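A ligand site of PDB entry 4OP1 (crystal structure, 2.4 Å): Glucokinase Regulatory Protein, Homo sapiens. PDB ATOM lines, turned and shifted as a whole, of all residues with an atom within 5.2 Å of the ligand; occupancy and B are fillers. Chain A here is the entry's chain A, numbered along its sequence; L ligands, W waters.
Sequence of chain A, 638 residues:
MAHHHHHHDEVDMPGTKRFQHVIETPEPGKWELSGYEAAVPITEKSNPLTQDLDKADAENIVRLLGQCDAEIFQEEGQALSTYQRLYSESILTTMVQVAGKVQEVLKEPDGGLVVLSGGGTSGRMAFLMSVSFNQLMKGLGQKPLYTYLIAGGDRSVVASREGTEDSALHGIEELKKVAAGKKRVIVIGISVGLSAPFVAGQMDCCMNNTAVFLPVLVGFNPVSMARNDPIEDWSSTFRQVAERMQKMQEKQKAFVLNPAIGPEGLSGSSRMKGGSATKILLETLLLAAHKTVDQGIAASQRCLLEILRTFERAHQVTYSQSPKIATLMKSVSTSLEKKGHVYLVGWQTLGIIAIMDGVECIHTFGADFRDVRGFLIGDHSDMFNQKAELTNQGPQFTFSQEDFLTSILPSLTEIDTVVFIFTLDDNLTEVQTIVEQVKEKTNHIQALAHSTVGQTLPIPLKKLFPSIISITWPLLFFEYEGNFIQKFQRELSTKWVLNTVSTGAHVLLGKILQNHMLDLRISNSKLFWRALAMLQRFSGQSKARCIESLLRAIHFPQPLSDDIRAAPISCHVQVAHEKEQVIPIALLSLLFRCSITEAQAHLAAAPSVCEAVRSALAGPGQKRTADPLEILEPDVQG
A nitrogen (N1) of the ligand sits at hydrogen-bond distance from the backbone carbonyl oxygen (O) of Gly 193 (2.8 Å).
The backbone carbonyl oxygen of Met 225 is in hydrogen-bond range of a nitrogen (N1) of the ligand (2.9 Å).
The backbone NH (N) of Arg 227 lies close to a nitrogen (N1) of the ligand, 3.3 Å away.
A ring nitrogen (ND1) of His 516 lies close to a fluorine (F1) of the ligand (3.2 Å).
A fluorine (F2) of the ligand lies close to the backbone carbonyl oxygen (O) of Ala 533 (3.1 Å).
The backbone NH (N) of Met 534 lies close to a fluorine (F2) of the ligand.
F3 of the ligand lies close to NE of Arg 537.
Tyr 36 touches the ligand (OH to C12, 3.9 Å).
CG1 of Val 40 touches C12 of the ligand (3.8 Å).
Pro 41 touches the ligand (CG to N2, 3.3 Å).
Glu 44 touches the ligand.
Ser 46 touches the ligand.
Ser 195 touches the ligand.
ND2 of Asn 221 touches N1 of the ligand, 3.7 Å away.
C of Ala 226 touches N1 of the ligand, 3.8 Å away.
O of Lys 526 touches C7 of the ligand (3.5 Å).
Trp 529 touches the ligand (CD1 to O1, 3.4 Å).
CA of Arg 530 touches C8 of the ligand (3.3 Å).
Hydrophobic or aromatic side chains that line the ligand: Val 40, Pro 41, His 516, Trp 529, Ala 533 and Met 534.
18 residues have an atom within 4 Å of the ligand: Tyr 36, Val 40, Pro 41, Glu 44, Ser 46, Gly 193, Ser 195, Asn 221, Met 225, Ala 226, Arg 227, His 516, Lys 526, Trp 529, Arg 530, Ala 533, Met 534 and Arg 537.
The nearest printed residue that does not touch the ligand is Lys 45 (4.2 Å).
Water W2 lies within hydrogen-bond range of OH of Tyr 36 (2.5 Å), O of Ala 533 (2.7 Å) and O3 of the ligand (2.7 Å).
Water W4 lies within hydrogen-bond range of OD1 of Asp 229, O2 of the ligand and NE2 of His 21.
Water W3 bridges a nitrogen (N2) of the ligand (2.9 Å) and the backbone carbonyl oxygen (O) of Met 225 (3.3 Å).
Water W1 lies within hydrogen-bond range of OE1 of Glu 44 (2.8 Å), N3 of the ligand (3.3 Å) and NE of Arg 530 (3.4 Å).
The side-chain hydroxyl (OG) of Ser 267 is in hydrogen-bond range of a ring nitrogen (ND1) of His 516, at 3.2 Å.
The backbone carbonyl oxygen (O) of Gly 193 is in hydrogen-bond range of the side-chain amide nitrogen (ND2) of Asn 221.
NE of Arg 530 is in salt-bridge range of OE1 of Glu 44 (2.7 Å).
The indole nitrogen (NE1) of Trp 529 sits at hydrogen-bond distance from the side-chain carboxylate (OD2) of Asp 229 (2.9 Å).
The side-chain carboxylate (OD2) of Asp 229 is in salt-bridge range of the guanidinium group (NH2) of Arg 227.
ND2 of Asn 221 lies within hydrogen-bond range of OG1 of Thr 43 (2.8 Å).
NH2 of Arg 227 sits at hydrogen-bond distance from OG of Ser 525 (2.8 Å).
OG of Ser 195 lies within hydrogen-bond range of NH1 of Arg 227 (3.1 Å).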
ATOM      1  N   HIS A  21       9.656  27.993   6.287  1.00  0.00           N
ATOM      2  CA  HIS A  21       9.243  27.047   7.325  1.00  0.00           C
ATOM      3  C   HIS A  21       7.827  27.296   7.869  1.00  0.00           C
ATOM      4  O   HIS A  21       7.266  26.431   8.486  1.00  0.00           O
ATOM      5  CB  HIS A  21      10.222  27.132   8.469  1.00  0.00           C
ATOM      6  CG  HIS A  21      10.073  28.392   9.273  1.00  0.00           C
ATOM      7  ND1 HIS A  21      10.615  29.593   8.857  1.00  0.00           N
ATOM      8  CD2 HIS A  21       9.414  28.646  10.423  1.00  0.00           C
ATOM      9  CE1 HIS A  21      10.316  30.526   9.748  1.00  0.00           C
ATOM     10  NE2 HIS A  21       9.589  29.973  10.709  1.00  0.00           N
ATOM     11  N   TYR A  36      -0.960  22.037  10.073  1.00  0.00           N
ATOM     12  CA  TYR A  36      -0.450  23.195  10.777  1.00  0.00           C
ATOM     13  C   TYR A  36      -0.282  22.935  12.248  1.00  0.00           C
ATOM     14  O   TYR A  36       0.783  23.223  12.776  1.00  0.00           O
ATOM     15  CB  TYR A  36      -1.396  24.393  10.634  1.00  0.00           C
ATOM     16  CG  TYR A  36      -0.861  25.603  11.308  1.00  0.00           C
ATOM     17  CD1 TYR A  36      -1.099  25.838  12.661  1.00  0.00           C
ATOM     18  CD2 TYR A  36      -0.069  26.513  10.628  1.00  0.00           C
ATOM     19  CE1 TYR A  36      -0.583  26.955  13.308  1.00  0.00           C
ATOM     20  CE2 TYR A  36       0.445  27.647  11.258  1.00  0.00           C
ATOM     21  CZ  TYR A  36       0.194  27.857  12.598  1.00  0.00           C
ATOM     22  OH  TYR A  36       0.705  28.938  13.248  1.00  0.00           O
ATOM     23  N   VAL A  40       2.767  22.570  15.462  1.00  0.00           N
ATOM     24  CA  VAL A  40       2.997  23.610  16.486  1.00  0.00           C
ATOM     25  C   VAL A  40       3.706  22.904  17.578  1.00  0.00           C
ATOM     26  O   VAL A  40       3.148  21.971  18.152  1.00  0.00           O
ATOM     27  CB  VAL A  40       1.703  24.263  17.030  1.00  0.00           C
ATOM     28  CG1 VAL A  40       1.976  25.165  18.238  1.00  0.00           C
ATOM     29  CG2 VAL A  40       0.998  25.041  15.937  1.00  0.00           C
ATOM     30  N   PRO A  41       4.945  23.306  17.878  1.00  0.00           N
ATOM     31  CA  PRO A  41       5.654  22.614  18.966  1.00  0.00           C
ATOM     32  C   PRO A  41       4.824  22.600  20.238  1.00  0.00           C
ATOM     33  O   PRO A  41       4.056  23.524  20.491  1.00  0.00           O
ATOM     34  CB  PRO A  41       6.948  23.413  19.122  1.00  0.00           C
ATOM     35  CG  PRO A  41       7.075  24.228  17.873  1.00  0.00           C
ATOM     36  CD  PRO A  41       5.699  24.481  17.380  1.00  0.00           C
ATOM     37  N   THR A  43       5.501  23.297  23.125  1.00  0.00           N
ATOM     38  CA  THR A  43       5.792  24.425  24.014  1.00  0.00           C
ATOM     39  C   THR A  43       5.090  25.669  23.592  1.00  0.00           C
ATOM     40  O   THR A  43       4.883  26.528  24.399  1.00  0.00           O
ATOM     41  CB  THR A  43       7.284  24.682  24.116  1.00  0.00           C
ATOM     42  OG1 THR A  43       7.817  24.901  22.805  1.00  0.00           O
ATOM     43  CG2 THR A  43       7.998  23.451  24.719  1.00  0.00           C
ATOM     44  N   GLU A  44       4.660  25.749  22.324  1.00  0.00           N
ATOM     45  CA  GLU A  44       3.949  26.922  21.852  1.00  0.00           C
ATOM     46  C   GLU A  44       2.465  26.727  21.730  1.00  0.00           C
ATOM     47  O   GLU A  44       1.766  27.681  21.405  1.00  0.00           O
ATOM     48  CB  GLU A  44       4.485  27.369  20.483  1.00  0.00           C
ATOM     49  CG  GLU A  44       5.947  27.703  20.516  1.00  0.00           C
ATOM     50  CD  GLU A  44       6.280  28.982  21.269  1.00  0.00           C
ATOM     51  OE1 GLU A  44       5.465  29.939  21.358  1.00  0.00           O
ATOM     52  OE2 GLU A  44       7.402  29.046  21.759  1.00  0.00           O
ATOM     53  N   LYS A  45       1.989  25.513  21.987  1.00  0.00           N
ATOM     54  CA  LYS A  45       0.577  25.186  21.817  1.00  0.00           C
ATOM     55  C   LYS A  45      -0.244  25.993  22.805  1.00  0.00           C
ATOM     56  O   LYS A  45       0.278  26.556  23.794  1.00  0.00           O
ATOM     57  CB  LYS A  45       0.307  23.654  22.014  1.00  0.00           C
ATOM     58  CG  LYS A  45       0.680  22.735  20.822  1.00  0.00           C
ATOM     59  CD  LYS A  45       0.091  21.326  20.971  1.00  0.00           C
ATOM     60  CE  LYS A  45       0.775  20.254  20.146  1.00  0.00           C
ATOM     61  NZ  LYS A  45       0.729  20.549  18.680  1.00  0.00           N
ATOM     62  N   SER A  46      -1.527  26.103  22.467  1.00  0.00           N
ATOM     63  CA  SER A  46      -2.505  26.667  23.367  1.00  0.00           C
ATOM     64  C   SER A  46      -2.994  25.533  24.258  1.00  0.00           C
ATOM     65  O   SER A  46      -3.492  24.536  23.751  1.00  0.00           O
ATOM     66  CB  SER A  46      -3.693  27.253  22.585  1.00  0.00           C
ATOM     67  OG  SER A  46      -4.884  27.151  23.369  1.00  0.00           O
ATOM     68  N   GLY A 193      12.097  25.310  24.612  1.00  0.00           N
ATOM     69  CA  GLY A 193      11.572  25.078  23.294  1.00  0.00           C
ATOM     70  C   GLY A 193      12.467  24.320  22.351  1.00  0.00           C
ATOM     71  O   GLY A 193      12.073  24.086  21.227  1.00  0.00           O
ATOM     72  N   LEU A 194      13.631  23.895  22.790  1.00  0.00           N
ATOM     73  CA  LEU A 194      14.676  23.425  21.875  1.00  0.00           C
ATOM     74  C   LEU A 194      14.802  24.475  20.765  1.00  0.00           C
ATOM     75  O   LEU A 194      14.695  24.185  19.609  1.00  0.00           O
ATOM     76  CB  LEU A 194      14.334  22.058  21.312  1.00  0.00           C
ATOM     77  CG  LEU A 194      14.245  20.841  22.255  1.00  0.00           C
ATOM     78  CD1 LEU A 194      14.228  19.536  21.469  1.00  0.00           C
ATOM     79  CD2 LEU A 194      15.404  20.795  23.213  1.00  0.00           C
ATOM     80  N   SER A 195      15.037  25.716  21.174  1.00  0.00           N
ATOM     81  CA  SER A 195      14.865  26.872  20.350  1.00  0.00           C
ATOM     82  C   SER A 195      16.060  27.797  20.280  1.00  0.00           C
ATOM     83  O   SER A 195      16.324  28.339  19.215  1.00  0.00           O
ATOM     84  CB  SER A 195      13.677  27.704  20.871  1.00  0.00           C
ATOM     85  OG  SER A 195      13.788  29.051  20.397  1.00  0.00           O
ATOM     86  N   ASN A 221      10.277  19.630  24.199  1.00  0.00           N
ATOM     87  CA  ASN A 221       9.644  19.262  22.940  1.00  0.00           C
ATOM     88  C   ASN A 221      10.335  18.021  22.390  1.00  0.00           C
ATOM     89  O   ASN A 221      11.521  17.818  22.620  1.00  0.00           O
ATOM     90  CB  ASN A 221       9.859  20.365  21.918  1.00  0.00           C
ATOM     91  CG  ASN A 221       8.889  21.483  22.036  1.00  0.00           C
ATOM     92  OD1 ASN A 221       7.710  21.254  22.230  1.00  0.00           O
ATOM     93  ND2 ASN A 221       9.381  22.736  21.887  1.00  0.00           N
ATOM     94  N   MET A 225      10.225  18.291  16.819  1.00  0.00           N
ATOM     95  CA  MET A 225       9.568  19.601  16.904  1.00  0.00           C
ATOM     96  C   MET A 225      10.572  20.670  17.269  1.00  0.00           C
ATOM     97  O   MET A 225      10.188  21.829  17.510  1.00  0.00           O
ATOM     98  CB  MET A 225       8.480  19.598  17.975  1.00  0.00           C
ATOM     99  CG  MET A 225       7.116  19.148  17.518  1.00  0.00           C
ATOM    100  SD  MET A 225       6.093  18.745  18.957  1.00  0.00           S
ATOM    101  CE  MET A 225       4.559  18.380  18.135  1.00  0.00           C
ATOM    102  N   ALA A 226      11.853  20.321  17.326  1.00  0.00           N
ATOM    103  CA  ALA A 226      12.856  21.297  17.663  1.00  0.00           C
ATOM    104  C   ALA A 226      12.852  22.358  16.592  1.00  0.00           C
ATOM    105  O   ALA A 226      12.550  22.096  15.458  1.00  0.00           O
ATOM    106  CB  ALA A 226      14.201  20.652  17.748  1.00  0.00           C
ATOM    107  N   ARG A 227      13.178  23.575  16.977  1.00  0.00           N
ATOM    108  CA  ARG A 227      13.167  24.718  16.073  1.00  0.00           C
ATOM    109  C   ARG A 227      13.991  24.426  14.827  1.00  0.00           C
ATOM    110  O   ARG A 227      15.100  23.851  14.936  1.00  0.00           O
ATOM    111  CB  ARG A 227      13.697  25.929  16.814  1.00  0.00           C
ATOM    112  CG  ARG A 227      12.991  27.174  16.460  1.00  0.00           C
ATOM    113  CD  ARG A 227      13.488  28.342  17.273  1.00  0.00           C
ATOM    114  NE  ARG A 227      13.569  29.530  16.426  1.00  0.00           N
ATOM    115  CZ  ARG A 227      13.913  30.757  16.819  1.00  0.00           C
ATOM    116  NH1 ARG A 227      14.182  31.026  18.086  1.00  0.00           N
ATOM    117  NH2 ARG A 227      13.996  31.728  15.913  1.00  0.00           N
ATOM    118  N   ASN A 228      13.429  24.758  13.664  1.00  0.00           N
ATOM    119  CA  ASN A 228      14.069  24.500  12.374  1.00  0.00           C
ATOM    120  C   ASN A 228      14.262  25.650  11.376  1.00  0.00           C
ATOM    121  O   ASN A 228      14.674  25.399  10.245  1.00  0.00           O
ATOM    122  CB  ASN A 228      13.372  23.318  11.659  1.00  0.00           C
ATOM    123  CG  ASN A 228      14.287  22.629  10.631  1.00  0.00           C
ATOM    124  OD1 ASN A 228      15.451  22.277  10.914  1.00  0.00           O
ATOM    125  ND2 ASN A 228      13.770  22.449   9.447  1.00  0.00           N
ATOM    126  N   ASP A 229      14.015  26.900  11.772  1.00  0.00           N
ATOM    127  CA  ASP A 229      14.312  28.086  10.946  1.00  0.00           C
ATOM    128  C   ASP A 229      15.765  28.483  11.066  1.00  0.00           C
ATOM    129  O   ASP A 229      16.332  28.310  12.128  1.00  0.00           O
ATOM    130  CB  ASP A 229      13.433  29.302  11.285  1.00  0.00           C
ATOM    131  CG  ASP A 229      13.377  29.621  12.786  1.00  0.00           C
ATOM    132  OD1 ASP A 229      13.064  28.711  13.617  1.00  0.00           O
ATOM    133  OD2 ASP A 229      13.584  30.806  13.144  1.00  0.00           O
ATOM    134  N   SER A 267       0.122  30.700  26.772  1.00  0.00           N
ATOM    135  CA  SER A 267       0.763  30.114  25.633  1.00  0.00           C
ATOM    136  C   SER A 267       2.180  30.604  25.465  1.00  0.00           C
ATOM    137  O   SER A 267       2.408  31.794  25.398  1.00  0.00           O
ATOM    138  CB  SER A 267      -0.067  30.360  24.390  1.00  0.00           C
ATOM    139  OG  SER A 267      -1.387  29.866  24.591  1.00  0.00           O
ATOM    140  N   HIS A 516      -3.467  33.858  25.322  1.00  0.00           N
ATOM    141  CA  HIS A 516      -2.335  34.374  24.582  1.00  0.00           C
ATOM    142  C   HIS A 516      -2.039  35.802  25.035  1.00  0.00           C
ATOM    143  O   HIS A 516      -2.977  36.576  25.326  1.00  0.00           O
ATOM    144  CB  HIS A 516      -2.688  34.398  23.087  1.00  0.00           C
ATOM    145  CG  HIS A 516      -3.060  33.052  22.526  1.00  0.00           C
ATOM    146  ND1 HIS A 516      -2.142  32.037  22.356  1.00  0.00           N
ATOM    147  CD2 HIS A 516      -4.242  32.568  22.076  1.00  0.00           C
ATOM    148  CE1 HIS A 516      -2.750  30.984  21.843  1.00  0.00           C
ATOM    149  NE2 HIS A 516      -4.030  31.270  21.670  1.00  0.00           N
ATOM    150  N   SER A 525      13.764  36.659  17.646  1.00  0.00           N
ATOM    151  CA  SER A 525      13.203  36.012  16.487  1.00  0.00           C
ATOM    152  C   SER A 525      12.072  35.075  16.845  1.00  0.00           C
ATOM    153  O   SER A 525      11.021  35.057  16.198  1.00  0.00           O
ATOM    154  CB  SER A 525      14.321  35.256  15.804  1.00  0.00           C
ATOM    155  OG  SER A 525      14.900  34.259  16.656  1.00  0.00           O
ATOM    156  N   LYS A 526      12.256  34.266  17.885  1.00  0.00           N
ATOM    157  CA  LYS A 526      11.150  33.488  18.460  1.00  0.00           C
ATOM    158  C   LYS A 526       9.855  34.272  18.657  1.00  0.00           C
ATOM    159  O   LYS A 526       8.772  33.798  18.334  1.00  0.00           O
ATOM    160  CB  LYS A 526      11.563  32.852  19.775  1.00  0.00           C
ATOM    161  CG  LYS A 526      10.472  32.020  20.428  1.00  0.00           C
ATOM    162  CD  LYS A 526      10.980  31.123  21.572  1.00  0.00           C
ATOM    163  CE  LYS A 526      11.550  31.943  22.724  1.00  0.00           C
ATOM    164  NZ  LYS A 526      12.054  31.036  23.760  1.00  0.00           N
ATOM    165  N   TRP A 529       8.242  35.009  15.394  1.00  0.00           N
ATOM    166  CA  TRP A 529       7.418  33.870  14.914  1.00  0.00           C
ATOM    167  C   TRP A 529       6.139  33.761  15.683  1.00  0.00           C
ATOM    168  O   TRP A 529       5.098  33.553  15.058  1.00  0.00           O
ATOM    169  CB  TRP A 529       8.179  32.533  14.825  1.00  0.00           C
ATOM    170  CG  TRP A 529       9.395  32.688  13.951  1.00  0.00           C
ATOM    171  CD1 TRP A 529      10.655  32.568  14.348  1.00  0.00           C
ATOM    172  CD2 TRP A 529       9.438  33.086  12.574  1.00  0.00           C
ATOM    173  NE1 TRP A 529      11.505  32.818  13.310  1.00  0.00           N
ATOM    174  CE2 TRP A 529      10.776  33.135  12.205  1.00  0.00           C
ATOM    175  CE3 TRP A 529       8.456  33.369  11.611  1.00  0.00           C
ATOM    176  CZ2 TRP A 529      11.209  33.468  10.894  1.00  0.00           C
ATOM    177  CZ3 TRP A 529       8.875  33.718  10.277  1.00  0.00           C
ATOM    178  CH2 TRP A 529      10.258  33.772   9.957  1.00  0.00           C
ATOM    179  N   ARG A 530       6.183  33.967  17.020  1.00  0.00           N
ATOM    180  CA  ARG A 530       4.973  33.909  17.842  1.00  0.00           C
ATOM    181  C   ARG A 530       3.971  34.973  17.411  1.00  0.00           C
ATOM    182  O   ARG A 530       2.767  34.731  17.358  1.00  0.00           O
ATOM    183  CB  ARG A 530       5.277  34.077  19.327  1.00  0.00           C
ATOM    184  CG  ARG A 530       4.063  33.766  20.212  1.00  0.00           C
ATOM    185  CD  ARG A 530       4.411  33.525  21.678  1.00  0.00           C
ATOM    186  NE  ARG A 530       5.507  32.564  21.848  1.00  0.00           N
ATOM    187  CZ  ARG A 530       6.481  32.650  22.777  1.00  0.00           C
ATOM    188  NH1 ARG A 530       6.544  33.676  23.636  1.00  0.00           N
ATOM    189  NH2 ARG A 530       7.432  31.723  22.832  1.00  0.00           N
ATOM    190  N   ALA A 533       2.369  33.775  14.028  1.00  0.00           N
ATOM    191  CA  ALA A 533       1.395  32.747  14.378  1.00  0.00           C
ATOM    192  C   ALA A 533       0.105  33.274  15.009  1.00  0.00           C
ATOM    193  O   ALA A 533      -1.022  32.817  14.703  1.00  0.00           O
ATOM    194  CB  ALA A 533       2.023  31.743  15.320  1.00  0.00           C
ATOM    195  N   MET A 534       0.235  34.243  15.895  1.00  0.00           N
ATOM    196  CA  MET A 534      -0.962  34.794  16.516  1.00  0.00           C
ATOM    197  C   MET A 534      -1.803  35.551  15.514  1.00  0.00           C
ATOM    198  O   MET A 534      -3.024  35.456  15.537  1.00  0.00           O
ATOM    199  CB  MET A 534      -0.605  35.640  17.691  1.00  0.00           C
ATOM    200  CG  MET A 534      -0.233  34.775  18.866  1.00  0.00           C
ATOM    201  SD  MET A 534      -0.010  35.770  20.331  1.00  0.00           S
ATOM    202  CE  MET A 534       1.321  36.852  19.908  1.00  0.00           C
ATOM    203  N   ARG A 537      -3.678  32.903  13.579  1.00  0.00           N
ATOM    204  CA  ARG A 537      -4.703  32.301  14.399  1.00  0.00           C
ATOM    205  C   ARG A 537      -5.928  33.193  14.615  1.00  0.00           C
ATOM    206  O   ARG A 537      -7.049  32.726  14.492  1.00  0.00           O
ATOM    207  CB  ARG A 537      -4.109  31.876  15.753  1.00  0.00           C
ATOM    208  CG  ARG A 537      -5.119  31.574  16.873  1.00  0.00           C
ATOM    209  CD  ARG A 537      -5.902  30.288  16.671  1.00  0.00           C
ATOM    210  NE  ARG A 537      -5.016  29.138  16.805  1.00  0.00           N
ATOM    211  CZ  ARG A 537      -5.380  27.867  16.668  1.00  0.00           C
ATOM    212  NH1 ARG A 537      -6.659  27.569  16.382  1.00  0.00           N
ATOM    213  NH2 ARG A 537      -4.456  26.905  16.796  1.00  0.00           N
HETATM  214  C1  LIG L   1       9.937  27.873  18.495  1.00  0.00           C
HETATM  215  C2  LIG L   1      10.274  26.669  19.049  1.00  0.00           C
HETATM  216  C3  LIG L   1      10.251  25.542  18.281  1.00  0.00           C
HETATM  217  N1  LIG L   1      10.600  24.400  18.852  1.00  0.00           N
HETATM  218  N2  LIG L   1       9.898  25.600  16.967  1.00  0.00           N
HETATM  219  C4  LIG L   1       9.533  26.761  16.418  1.00  0.00           C
HETATM  220  C5  LIG L   1       9.571  27.933  17.161  1.00  0.00           C
HETATM  221  S1  LIG L   1       9.073  29.452  16.483  1.00  0.00           S
HETATM  222  O1  LIG L   1       9.916  30.523  16.978  1.00  0.00           O
HETATM  223  O2  LIG L   1       9.142  29.144  15.058  1.00  0.00           O
HETATM  224  C6  LIG L   1       7.520  29.781  17.014  1.00  0.00           C
HETATM  225  S2  LIG L   1       6.128  28.943  16.514  1.00  0.00           S
HETATM  226  C7  LIG L   1       7.236  30.721  17.935  1.00  0.00           C
HETATM  227  C8  LIG L   1       5.924  30.762  18.218  1.00  0.00           C
HETATM  228  C9  LIG L   1       5.140  29.881  17.530  1.00  0.00           C
HETATM  229  C10 LIG L   1       3.754  29.712  17.637  1.00  0.00           C
HETATM  230  C11 LIG L   1       3.025  28.836  16.805  1.00  0.00           C
HETATM  231  C12 LIG L   1       1.653  28.702  16.995  1.00  0.00           C
HETATM  232 CL1  LIG L   1       3.777  27.885  15.512  1.00  0.00          CL
HETATM  233  N3  LIG L   1       3.118  30.398  18.606  1.00  0.00           N
HETATM  234  C13 LIG L   1       1.792  30.279  18.796  1.00  0.00           C
HETATM  235  C14 LIG L   1       1.019  29.443  17.988  1.00  0.00           C
HETATM  236  C15 LIG L   1      -0.477  29.277  18.219  1.00  0.00           C
HETATM  237  C16 LIG L   1      -1.205  30.556  18.398  1.00  0.00           C
HETATM  238  F1  LIG L   1      -0.818  30.985  19.583  1.00  0.00           F
HETATM  239  F2  LIG L   1      -0.932  31.441  17.467  1.00  0.00           F
HETATM  240  F3  LIG L   1      -2.478  30.214  18.336  1.00  0.00           F
HETATM  241  C17 LIG L   1      -0.720  28.500  19.522  1.00  0.00           C
HETATM  242  O3  LIG L   1      -1.030  28.681  17.090  1.00  0.00           O
HETATM  243  O   HOH W   1       2.807  30.487  21.937  1.00  0.00           O
HETATM  244  O   HOH W   2      -0.878  30.112  14.785  1.00  0.00           O
HETATM  245  O   HOH W   3       9.277  23.659  14.889  1.00  0.00           O
HETATM  246  O   HOH W   4      10.702  27.842  13.157  1.00  0.00           O
